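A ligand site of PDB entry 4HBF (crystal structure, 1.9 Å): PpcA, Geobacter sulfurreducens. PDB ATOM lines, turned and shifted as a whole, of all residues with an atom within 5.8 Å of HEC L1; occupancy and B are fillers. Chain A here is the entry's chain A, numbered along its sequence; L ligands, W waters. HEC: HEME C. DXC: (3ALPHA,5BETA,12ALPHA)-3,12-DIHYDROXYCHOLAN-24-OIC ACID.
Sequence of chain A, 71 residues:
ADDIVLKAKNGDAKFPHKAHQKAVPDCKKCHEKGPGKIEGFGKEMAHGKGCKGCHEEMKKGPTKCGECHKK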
ATOM      1  N   ALA A   1       8.597 -19.623  18.824  1.00  0.00           N
ATOM      2  CA  ALA A   1       9.464 -19.857  20.028  1.00  0.00           C
ATOM      3  C   ALA A   1       8.901 -19.149  21.240  1.00  0.00           C
ATOM      4  O   ALA A   1       8.008 -18.312  21.126  1.00  0.00           O
ATOM      5  CB  ALA A   1      10.884 -19.406  19.771  1.00  0.00           C
ATOM      6  N   ASP A   2       9.461 -19.473  22.397  1.00  0.00           N
ATOM      7  CA  ASP A   2       8.988 -18.949  23.660  1.00  0.00           C
ATOM      8  C   ASP A   2       9.750 -17.717  24.076  1.00  0.00           C
ATOM      9  O   ASP A   2      10.911 -17.544  23.704  1.00  0.00           O
ATOM     10  CB  ASP A   2       9.157 -20.003  24.746  1.00  0.00           C
ATOM     11  CG  ASP A   2       8.281 -21.180  24.517  1.00  0.00           C
ATOM     12  OD1 ASP A   2       7.045 -20.945  24.350  1.00  0.00           O
ATOM     13  OD2 ASP A   2       8.746 -22.359  24.476  1.00  0.00           O
ATOM     14  N   ASP A   3       9.085 -16.867  24.856  1.00  0.00           N
ATOM     15  CA  ASP A   3       9.756 -15.746  25.509  1.00  0.00           C
ATOM     16  C   ASP A   3      10.802 -16.297  26.453  1.00  0.00           C
ATOM     17  O   ASP A   3      10.777 -17.478  26.785  1.00  0.00           O
ATOM     18  CB  ASP A   3       8.763 -14.900  26.264  1.00  0.00           C
ATOM     19  CG  ASP A   3       7.874 -14.107  25.336  1.00  0.00           C
ATOM     20  OD1 ASP A   3       8.248 -13.898  24.155  1.00  0.00           O
ATOM     21  OD2 ASP A   3       6.806 -13.661  25.718  1.00  0.00           O
ATOM     22  N   ILE A   4      11.778 -15.461  26.802  1.00  0.00           N
ATOM     23  CA  ILE A   4      12.771 -15.904  27.732  1.00  0.00           C
ATOM     24  C   ILE A   4      12.756 -15.024  28.970  1.00  0.00           C
ATOM     25  O   ILE A   4      12.316 -13.895  28.930  1.00  0.00           O
ATOM     26  CB  ILE A   4      14.158 -15.952  27.084  1.00  0.00           C
ATOM     27  CG1 ILE A   4      14.428 -14.674  26.295  1.00  0.00           C
ATOM     28  CG2 ILE A   4      14.276 -17.176  26.163  1.00  0.00           C
ATOM     29  CD1 ILE A   4      15.768 -14.650  25.673  1.00  0.00           C
ATOM     30  N   PHE A  15      11.389 -11.054  28.986  1.00  0.00           N
ATOM     31  CA  PHE A  15      11.514 -10.373  27.720  1.00  0.00           C
ATOM     32  C   PHE A  15      10.393 -10.849  26.805  1.00  0.00           C
ATOM     33  O   PHE A  15      10.454 -11.985  26.287  1.00  0.00           O
ATOM     34  CB  PHE A  15      12.846 -10.693  27.070  1.00  0.00           C
ATOM     35  CG  PHE A  15      12.971 -10.108  25.694  1.00  0.00           C
ATOM     36  CD1 PHE A  15      13.182  -8.729  25.532  1.00  0.00           C
ATOM     37  CD2 PHE A  15      12.786 -10.906  24.568  1.00  0.00           C
ATOM     38  CE1 PHE A  15      13.257  -8.157  24.286  1.00  0.00           C
ATOM     39  CE2 PHE A  15      12.874 -10.343  23.303  1.00  0.00           C
ATOM     40  CZ  PHE A  15      13.105  -8.973  23.153  1.00  0.00           C
ATOM     41  N   PRO A  16       9.339 -10.049  26.646  1.00  0.00           N
ATOM     42  CA  PRO A  16       8.211 -10.435  25.781  1.00  0.00           C
ATOM     43  C   PRO A  16       8.459 -10.032  24.321  1.00  0.00           C
ATOM     44  O   PRO A  16       8.403  -8.854  23.983  1.00  0.00           O
ATOM     45  CB  PRO A  16       7.041  -9.688  26.413  1.00  0.00           C
ATOM     46  CG  PRO A  16       7.651  -8.443  26.925  1.00  0.00           C
ATOM     47  CD  PRO A  16       9.074  -8.785  27.337  1.00  0.00           C
ATOM     48  N   HIS A  17       8.724 -11.018  23.479  1.00  0.00           N
ATOM     49  CA  HIS A  17       9.113 -10.714  22.099  1.00  0.00           C
ATOM     50  C   HIS A  17       8.023 -10.041  21.292  1.00  0.00           C
ATOM     51  O   HIS A  17       8.294  -9.099  20.544  1.00  0.00           O
ATOM     52  CB  HIS A  17       9.588 -11.954  21.361  1.00  0.00           C
ATOM     53  CG  HIS A  17      10.176 -11.639  20.021  1.00  0.00           C
ATOM     54  ND1 HIS A  17       9.478 -11.797  18.844  1.00  0.00           N
ATOM     55  CD2 HIS A  17      11.361 -11.089  19.679  1.00  0.00           C
ATOM     56  CE1 HIS A  17      10.220 -11.398  17.837  1.00  0.00           C
ATOM     57  NE2 HIS A  17      11.380 -10.971  18.309  1.00  0.00           N
ATOM     58  N   HIS A  20       7.903  -6.383  21.421  1.00  0.00           N
ATOM     59  CA  HIS A  20       9.077  -5.781  20.798  1.00  0.00           C
ATOM     60  C   HIS A  20       9.043  -5.822  19.284  1.00  0.00           C
ATOM     61  O   HIS A  20       9.421  -4.855  18.628  1.00  0.00           O
ATOM     62  CB  HIS A  20      10.363  -6.423  21.310  1.00  0.00           C
ATOM     63  CG  HIS A  20      10.647  -6.068  22.746  1.00  0.00           C
ATOM     64  ND1 HIS A  20      10.161  -6.800  23.803  1.00  0.00           N
ATOM     65  CD2 HIS A  20      11.307  -5.026  23.285  1.00  0.00           C
ATOM     66  CE1 HIS A  20      10.535  -6.230  24.934  1.00  0.00           C
ATOM     67  NE2 HIS A  20      11.216  -5.139  24.657  1.00  0.00           N
ATOM     68  N   GLN A  21       8.619  -6.940  18.722  1.00  0.00           N
ATOM     69  CA  GLN A  21       8.455  -7.058  17.274  1.00  0.00           C
ATOM     70  C   GLN A  21       7.505  -5.963  16.759  1.00  0.00           C
ATOM     71  O   GLN A  21       7.724  -5.355  15.714  1.00  0.00           O
ATOM     72  CB  GLN A  21       7.877  -8.420  16.954  1.00  0.00           C
ATOM     73  CG  GLN A  21       7.974  -8.855  15.510  1.00  0.00           C
ATOM     74  CD  GLN A  21       7.938 -10.363  15.408  1.00  0.00           C
ATOM     75  OE1 GLN A  21       7.132 -11.010  16.056  1.00  0.00           O
ATOM     76  NE2 GLN A  21       8.837 -10.926  14.630  1.00  0.00           N
ATOM     77  N   LYS A  22       6.449  -5.695  17.545  1.00  0.00           N
ATOM     78  CA  LYS A  22       5.455  -4.674  17.195  1.00  0.00           C
ATOM     79  C   LYS A  22       5.957  -3.223  17.373  1.00  0.00           C
ATOM     80  O   LYS A  22       5.744  -2.354  16.489  1.00  0.00           O
ATOM     81  CB  LYS A  22       4.161  -4.908  17.980  1.00  0.00           C
ATOM     82  CG  LYS A  22       3.107  -3.856  17.718  1.00  0.00           C
ATOM     83  CD  LYS A  22       1.734  -4.250  18.216  1.00  0.00           C
ATOM     84  CE  LYS A  22       0.696  -3.269  17.692  1.00  0.00           C
ATOM     85  NZ  LYS A  22      -0.680  -3.677  18.070  1.00  0.00           N
ATOM     86  N   VAL A  24       9.149  -2.224  17.799  1.00  0.00           N
ATOM     87  CA  VAL A  24      10.488  -1.965  17.274  1.00  0.00           C
ATOM     88  C   VAL A  24      10.598  -2.631  15.876  1.00  0.00           C
ATOM     89  O   VAL A  24      11.260  -3.650  15.695  1.00  0.00           O
ATOM     90  CB  VAL A  24      11.608  -2.457  18.231  1.00  0.00           C
ATOM     91  CG1 VAL A  24      12.965  -1.983  17.765  1.00  0.00           C
ATOM     92  CG2 VAL A  24      11.385  -1.971  19.657  1.00  0.00           C
ATOM     93  N   PRO A  25       9.958  -2.012  14.877  1.00  0.00           N
ATOM     94  CA  PRO A  25      10.021  -2.491  13.487  1.00  0.00           C
ATOM     95  C   PRO A  25      11.424  -2.474  12.874  1.00  0.00           C
ATOM     96  O   PRO A  25      11.659  -3.163  11.899  1.00  0.00           O
ATOM     97  CB  PRO A  25       9.091  -1.503  12.750  1.00  0.00           C
ATOM     98  CG  PRO A  25       9.138  -0.237  13.623  1.00  0.00           C
ATOM     99  CD  PRO A  25       9.129  -0.795  15.018  1.00  0.00           C
ATOM    100  N   ASP A  26      12.349  -1.706  13.438  1.00  0.00           N
ATOM    101  CA  ASP A  26      13.742  -1.796  13.068  1.00  0.00           C
ATOM    102  C   ASP A  26      14.383  -3.031  13.754  1.00  0.00           C
ATOM    103  O   ASP A  26      15.133  -2.911  14.722  1.00  0.00           O
ATOM    104  CB  ASP A  26      14.478  -0.499  13.417  1.00  0.00           C
ATOM    105  CG  ASP A  26      15.916  -0.479  12.936  1.00  0.00           C
ATOM    106  OD1 ASP A  26      16.277  -1.296  12.059  1.00  0.00           O
ATOM    107  OD2 ASP A  26      16.782   0.309  13.426  1.00  0.00           O
ATOM    108  N   CYS A  27      14.136  -4.202  13.166  1.00  0.00           N
ATOM    109  CA  CYS A  27      14.587  -5.506  13.682  1.00  0.00           C
ATOM    110  C   CYS A  27      16.082  -5.559  13.855  1.00  0.00           C
ATOM    111  O   CYS A  27      16.554  -6.274  14.720  1.00  0.00           O
ATOM    112  CB  CYS A  27      14.174  -6.638  12.752  1.00  0.00           C
ATOM    113  SG  CYS A  27      12.460  -6.614  12.184  1.00  0.00           S
ATOM    114  N   LYS A  29      17.895  -3.527  15.172  1.00  0.00           N
ATOM    115  CA  LYS A  29      18.263  -3.081  16.520  1.00  0.00           C
ATOM    116  C   LYS A  29      18.734  -4.224  17.387  1.00  0.00           C
ATOM    117  O   LYS A  29      19.524  -4.013  18.279  1.00  0.00           O
ATOM    118  CB  LYS A  29      17.093  -2.385  17.185  1.00  0.00           C
ATOM    119  CG  LYS A  29      16.940  -0.936  16.774  1.00  0.00           C
ATOM    120  CD  LYS A  29      18.194  -0.153  17.145  1.00  0.00           C
ATOM    121  CE  LYS A  29      17.966   1.347  17.179  1.00  0.00           C
ATOM    122  NZ  LYS A  29      19.142   1.995  17.853  1.00  0.00           N
ATOM    123  N   CYS A  30      18.226  -5.421  17.137  1.00  0.00           N
ATOM    124  CA  CYS A  30      18.622  -6.610  17.895  1.00  0.00           C
ATOM    125  C   CYS A  30      19.114  -7.766  17.064  1.00  0.00           C
ATOM    126  O   CYS A  30      19.902  -8.586  17.549  1.00  0.00           O
ATOM    127  CB  CYS A  30      17.414  -7.104  18.668  1.00  0.00           C
ATOM    128  SG  CYS A  30      16.808  -5.884  19.839  1.00  0.00           S
ATOM    129  N   HIS A  31      18.614  -7.894  15.850  1.00  0.00           N
ATOM    130  CA  HIS A  31      18.930  -9.052  15.007  1.00  0.00           C
ATOM    131  C   HIS A  31      20.011  -8.728  13.972  1.00  0.00           C
ATOM    132  O   HIS A  31      20.282  -7.581  13.668  1.00  0.00           O
ATOM    133  CB  HIS A  31      17.669  -9.575  14.326  1.00  0.00           C
ATOM    134  CG  HIS A  31      16.685 -10.179  15.281  1.00  0.00           C
ATOM    135  ND1 HIS A  31      17.014 -11.196  16.144  1.00  0.00           N
ATOM    136  CD2 HIS A  31      15.391  -9.885  15.545  1.00  0.00           C
ATOM    137  CE1 HIS A  31      15.965 -11.530  16.881  1.00  0.00           C
ATOM    138  NE2 HIS A  31      14.963 -10.736  16.545  1.00  0.00           N
ATOM    139  N   GLY A  50      21.129  -2.310  25.931  1.00  0.00           N
ATOM    140  CA  GLY A  50      20.553  -3.646  25.831  1.00  0.00           C
ATOM    141  C   GLY A  50      19.077  -3.737  26.198  1.00  0.00           C
ATOM    142  O   GLY A  50      18.360  -4.548  25.625  1.00  0.00           O
HETATM  143 FE   HEC L   1      13.173 -10.878  17.392  1.00  0.00          FE
HETATM  144  CHA HEC L   1      13.230 -14.073  18.472  1.00  0.00           C
HETATM  145  CHB HEC L   1      12.193 -11.870  14.319  1.00  0.00           C
HETATM  146  CHC HEC L   1      12.455  -7.597  16.589  1.00  0.00           C
HETATM  147  CHD HEC L   1      14.946  -9.870  20.075  1.00  0.00           C
HETATM  148  NA  HEC L   1      12.863 -12.598  16.539  1.00  0.00           N
HETATM  149  C1A HEC L   1      12.796 -13.804  17.199  1.00  0.00           C
HETATM  150  C2A HEC L   1      12.167 -14.778  16.342  1.00  0.00           C
HETATM  151  C3A HEC L   1      11.879 -14.195  15.182  1.00  0.00           C
HETATM  152  C4A HEC L   1      12.313 -12.813  15.287  1.00  0.00           C
HETATM  153  CMA HEC L   1      11.209 -14.870  13.955  1.00  0.00           C
HETATM  154  CAA HEC L   1      11.789 -16.221  16.734  1.00  0.00           C
HETATM  155  CBA HEC L   1      10.340 -15.913  17.218  1.00  0.00           C
HETATM  156  CGA HEC L   1       9.441 -17.098  17.404  1.00  0.00           C
HETATM  157  O1A HEC L   1       9.702 -18.170  16.780  1.00  0.00           O
HETATM  158  O2A HEC L   1       8.446 -16.962  18.178  1.00  0.00           O
HETATM  159  NB  HEC L   1      12.442  -9.893  15.761  1.00  0.00           N
HETATM  160  C1B HEC L   1      12.094 -10.505  14.576  1.00  0.00           C
HETATM  161  C2B HEC L   1      11.627  -9.492  13.648  1.00  0.00           C
HETATM  162  C3B HEC L   1      11.696  -8.298  14.290  1.00  0.00           C
HETATM  163  C4B HEC L   1      12.207  -8.543  15.615  1.00  0.00           C
HETATM  164  CMB HEC L   1      11.138  -9.794  12.208  1.00  0.00           C
HETATM  165  CAB HEC L   1      11.320  -6.869  13.812  1.00  0.00           C
HETATM  166  CBB HEC L   1      10.026  -6.612  13.518  1.00  0.00           C
HETATM  167  NC  HEC L   1      13.588  -9.096  18.183  1.00  0.00           N
HETATM  168  C1C HEC L   1      13.222  -7.826  17.713  1.00  0.00           C
HETATM  169  C2C HEC L   1      13.792  -6.827  18.576  1.00  0.00           C
HETATM  170  C3C HEC L   1      14.471  -7.471  19.518  1.00  0.00           C
HETATM  171  C4C HEC L   1      14.365  -8.894  19.295  1.00  0.00           C
HETATM  172  CMC HEC L   1      13.643  -5.293  18.382  1.00  0.00           C
HETATM  173  CAC HEC L   1      15.269  -6.839  20.678  1.00  0.00           C
HETATM  174  CBC HEC L   1      14.652  -5.863  21.414  1.00  0.00           C
HETATM  175  ND  HEC L   1      13.995 -11.828  18.990  1.00  0.00           N
HETATM  176  C1D HEC L   1      14.696 -11.214  20.014  1.00  0.00           C
HETATM  177  C2D HEC L   1      15.067 -12.202  21.002  1.00  0.00           C
HETATM  178  C3D HEC L   1      14.525 -13.518  20.514  1.00  0.00           C
HETATM  179  C4D HEC L   1      13.891 -13.179  19.254  1.00  0.00           C
HETATM  180  CMD HEC L   1      15.852 -11.983  22.273  1.00  0.00           C
HETATM  181  CAD HEC L   1      14.621 -14.887  21.175  1.00  0.00           C
HETATM  182  CBD HEC L   1      13.831 -14.942  22.471  1.00  0.00           C
HETATM  183  CGD HEC L   1      12.349 -14.753  22.285  1.00  0.00           C
HETATM  184  O1D HEC L   1      11.803 -15.246  21.276  1.00  0.00           O
HETATM  185  O2D HEC L   1      11.736 -14.119  23.188  1.00  0.00           O
HETATM  186 FE   HEC L   2      11.777  -3.587  25.787  1.00  0.00          FE
HETATM  187  CHA HEC L   2       8.481  -2.893  26.094  1.00  0.00           C
HETATM  188  CHB HEC L   2      11.615  -5.545  28.614  1.00  0.00           C
HETATM  189  CHC HEC L   2      14.993  -4.604  25.315  1.00  0.00           C
HETATM  190  CHD HEC L   2      12.096  -1.423  23.191  1.00  0.00           C
HETATM  191  NA  HEC L   2      10.347  -4.112  27.093  1.00  0.00           N
HETATM  192  C1A HEC L   2       9.010  -3.752  27.013  1.00  0.00           C
HETATM  193  C2A HEC L   2       8.264  -4.448  28.031  1.00  0.00           C
HETATM  194  C3A HEC L   2       9.123  -5.177  28.738  1.00  0.00           C
HETATM  195  C4A HEC L   2      10.450  -4.969  28.174  1.00  0.00           C
HETATM  196  CMA HEC L   2       8.783  -6.102  29.918  1.00  0.00           C
HETATM  197  CAA HEC L   2       6.738  -4.343  28.290  1.00  0.00           C
HETATM  198  CBA HEC L   2       5.955  -5.025  27.183  1.00  0.00           C
HETATM  199  CGA HEC L   2       4.473  -4.732  27.311  1.00  0.00           C
HETATM  200  O1A HEC L   2       4.117  -3.641  27.792  1.00  0.00           O
HETATM  201  O2A HEC L   2       3.672  -5.629  26.959  1.00  0.00           O
HETATM  202  NB  HEC L   2      13.075  -4.857  26.772  1.00  0.00           N
HETATM  203  C1B HEC L   2      12.817  -5.520  27.946  1.00  0.00           C
HETATM  204  C2B HEC L   2      14.018  -6.217  28.331  1.00  0.00           C
HETATM  205  C3B HEC L   2      14.949  -5.985  27.398  1.00  0.00           C
HETATM  206  C4B HEC L   2      14.353  -5.110  26.416  1.00  0.00           C
HETATM  207  CMB HEC L   2      14.122  -7.055  29.604  1.00  0.00           C
HETATM  208  CAB HEC L   2      16.392  -6.514  27.339  1.00  0.00           C
HETATM  209  CBB HEC L   2      16.555  -7.855  27.506  1.00  0.00           C
HETATM  210  NC  HEC L   2      13.261  -3.104  24.520  1.00  0.00           N
HETATM  211  C1C HEC L   2      14.521  -3.630  24.490  1.00  0.00           C
HETATM  212  C2C HEC L   2      15.268  -3.045  23.395  1.00  0.00           C
HETATM  213  C3C HEC L   2      14.470  -2.160  22.802  1.00  0.00           C
HETATM  214  C4C HEC L   2      13.206  -2.169  23.500  1.00  0.00           C
HETATM  215  CMC HEC L   2      16.747  -3.394  23.075  1.00  0.00           C
HETATM  216  CAC HEC L   2      14.800  -1.275  21.570  1.00  0.00           C
HETATM  217  CBC HEC L   2      15.844  -1.563  20.780  1.00  0.00           C
HETATM  218  ND  HEC L   2      10.489  -2.361  24.791  1.00  0.00           N
HETATM  219  C1D HEC L   2      10.866  -1.511  23.762  1.00  0.00           C
HETATM  220  C2D HEC L   2       9.713  -0.712  23.381  1.00  0.00           C
HETATM  221  C3D HEC L   2       8.583  -1.180  24.278  1.00  0.00           C
HETATM  222  C4D HEC L   2       9.167  -2.198  25.130  1.00  0.00           C
HETATM  223  CMD HEC L   2       9.651   0.361  22.306  1.00  0.00           C
HETATM  224  CAD HEC L   2       7.141  -0.680  24.313  1.00  0.00           C
HETATM  225  CBD HEC L   2       6.216  -1.830  23.966  1.00  0.00           C
HETATM  226  CGD HEC L   2       4.773  -1.383  24.086  1.00  0.00           C
HETATM  227  O1D HEC L   2       4.385  -0.829  25.142  1.00  0.00           O
HETATM  228  O2D HEC L   2       4.040  -1.579  23.105  1.00  0.00           O
HETATM  229  C1  DXC L   3      21.645 -13.643  27.111  1.00  0.00           C
HETATM  230  C2  DXC L   3      20.410 -12.683  27.096  1.00  0.00           C
HETATM  231  C3  DXC L   3      19.455 -13.016  25.942  1.00  0.00           C
HETATM  232  C4  DXC L   3      20.171 -12.943  24.552  1.00  0.00           C
HETATM  233  C5  DXC L   3      21.427 -13.846  24.604  1.00  0.00           C
HETATM  234  C6  DXC L   3      22.347 -13.509  25.769  1.00  0.00           C
HETATM  235  C7  DXC L   3      18.205 -12.106  26.012  1.00  0.00           C
HETATM  236  C8  DXC L   3      18.532 -10.661  25.663  1.00  0.00           C
HETATM  237  C9  DXC L   3      19.230 -10.574  24.281  1.00  0.00           C
HETATM  238  C10 DXC L   3      20.497 -11.472  24.218  1.00  0.00           C
HETATM  239  C11 DXC L   3      19.597  -9.116  23.938  1.00  0.00           C
HETATM  240  C12 DXC L   3      20.199  -8.948  22.541  1.00  0.00           C
HETATM  241  C13 DXC L   3      21.489  -9.811  22.519  1.00  0.00           C
HETATM  242  C14 DXC L   3      21.217 -11.296  22.854  1.00  0.00           C
HETATM  243  C15 DXC L   3      18.454  -8.075  23.982  1.00  0.00           C
HETATM  244  C16 DXC L   3      18.939  -6.934  23.113  1.00  0.00           C
HETATM  245  C17 DXC L   3      20.313  -7.394  22.577  1.00  0.00           C
HETATM  246  C18 DXC L   3      19.258 -13.529  23.480  1.00  0.00           C
HETATM  247  C19 DXC L   3      20.635  -6.693  21.236  1.00  0.00           C
HETATM  248  O1  DXC L   3      22.463  -9.334  23.462  1.00  0.00           O
HETATM  249  O2  DXC L   3      22.532 -13.242  28.168  1.00  0.00           O
HETATM  250  C20 DXC L   3      19.269  -9.376  21.420  1.00  0.00           C
HETATM  251  C21 DXC L   3      20.574  -5.165  21.318  1.00  0.00           C
HETATM  252  C22 DXC L   3      21.589  -4.557  22.257  1.00  0.00           C
HETATM  253  C23 DXC L   3      22.849  -4.139  21.531  1.00  0.00           C
HETATM  254  O3  DXC L   3      22.853  -3.188  20.752  1.00  0.00           O
HETATM  255  O4  DXC L   3      23.888  -4.767  21.763  1.00  0.00           O
HETATM  256  C24 DXC L   3      21.976  -7.138  20.698  1.00  0.00           C
HETATM  257  O   HOH W   1       7.720 -19.311  15.654  1.00  0.00           O
HETATM  258  O   HOH W   2       9.173 -15.449  21.670  1.00  0.00           O
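A ring nitrogen (NE2) of His 31 binds an iron atom (FE) of HEC L1, at 2.0 Å.
The side-chain sulfur of Cys 30 is bonded to a carbon (CAC) of HEC L1.
SG of Cys 27 is covalently linked to CAB of HEC L1.
A ring nitrogen (NE2) of His 17 binds an iron atom (FE) of HEC L1, at 2.0 Å.
N of Ala 1 sits at hydrogen-bond distance from O1A of HEC L1 (2.7 Å).
FE of HEC L2 is bound by NE2 of His 20.
OD1 of Asp 3 is in hydrogen-bond range of N of His 17, 3.0 Å away.
The backbone NH (N) of Phe 15 is in hydrogen-bond range of the backbone carbonyl oxygen (O) of Ile 4 (3.0 Å).
A ring nitrogen (ND1) of His 20 is in hydrogen-bond range of the backbone carbonyl oxygen of Pro 16.
The backbone carbonyl oxygen of Asp 2 sits close to an oxygen (O1D) of HEC L1, at 3.5 Å.
Asp 3 touches HEC L1.
Ile 4 touches HEC L1.
CE2 of Phe 15 touches CMD of HEC L1, 3.6 Å away.
His 20 touches HEC L1 (CD2 to CBC, 3.9 Å).
Gln 21 touches HEC L1 (NE2 to C1B, 3.3 Å).
Val 24 touches HEC L1 (CG1 to CMC, 3.4 Å).
Hydrophobic or aromatic side chains within 4 Å of HEC L1: Ala 1, Ile 4, Phe 15, His 17, His 20, Val 24 and His 31.
Water W1 lies within hydrogen-bond range of an oxygen (O1A) of HEC L1 (2.5 Å) and the backbone NH of Ala 1 (3.3 Å).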
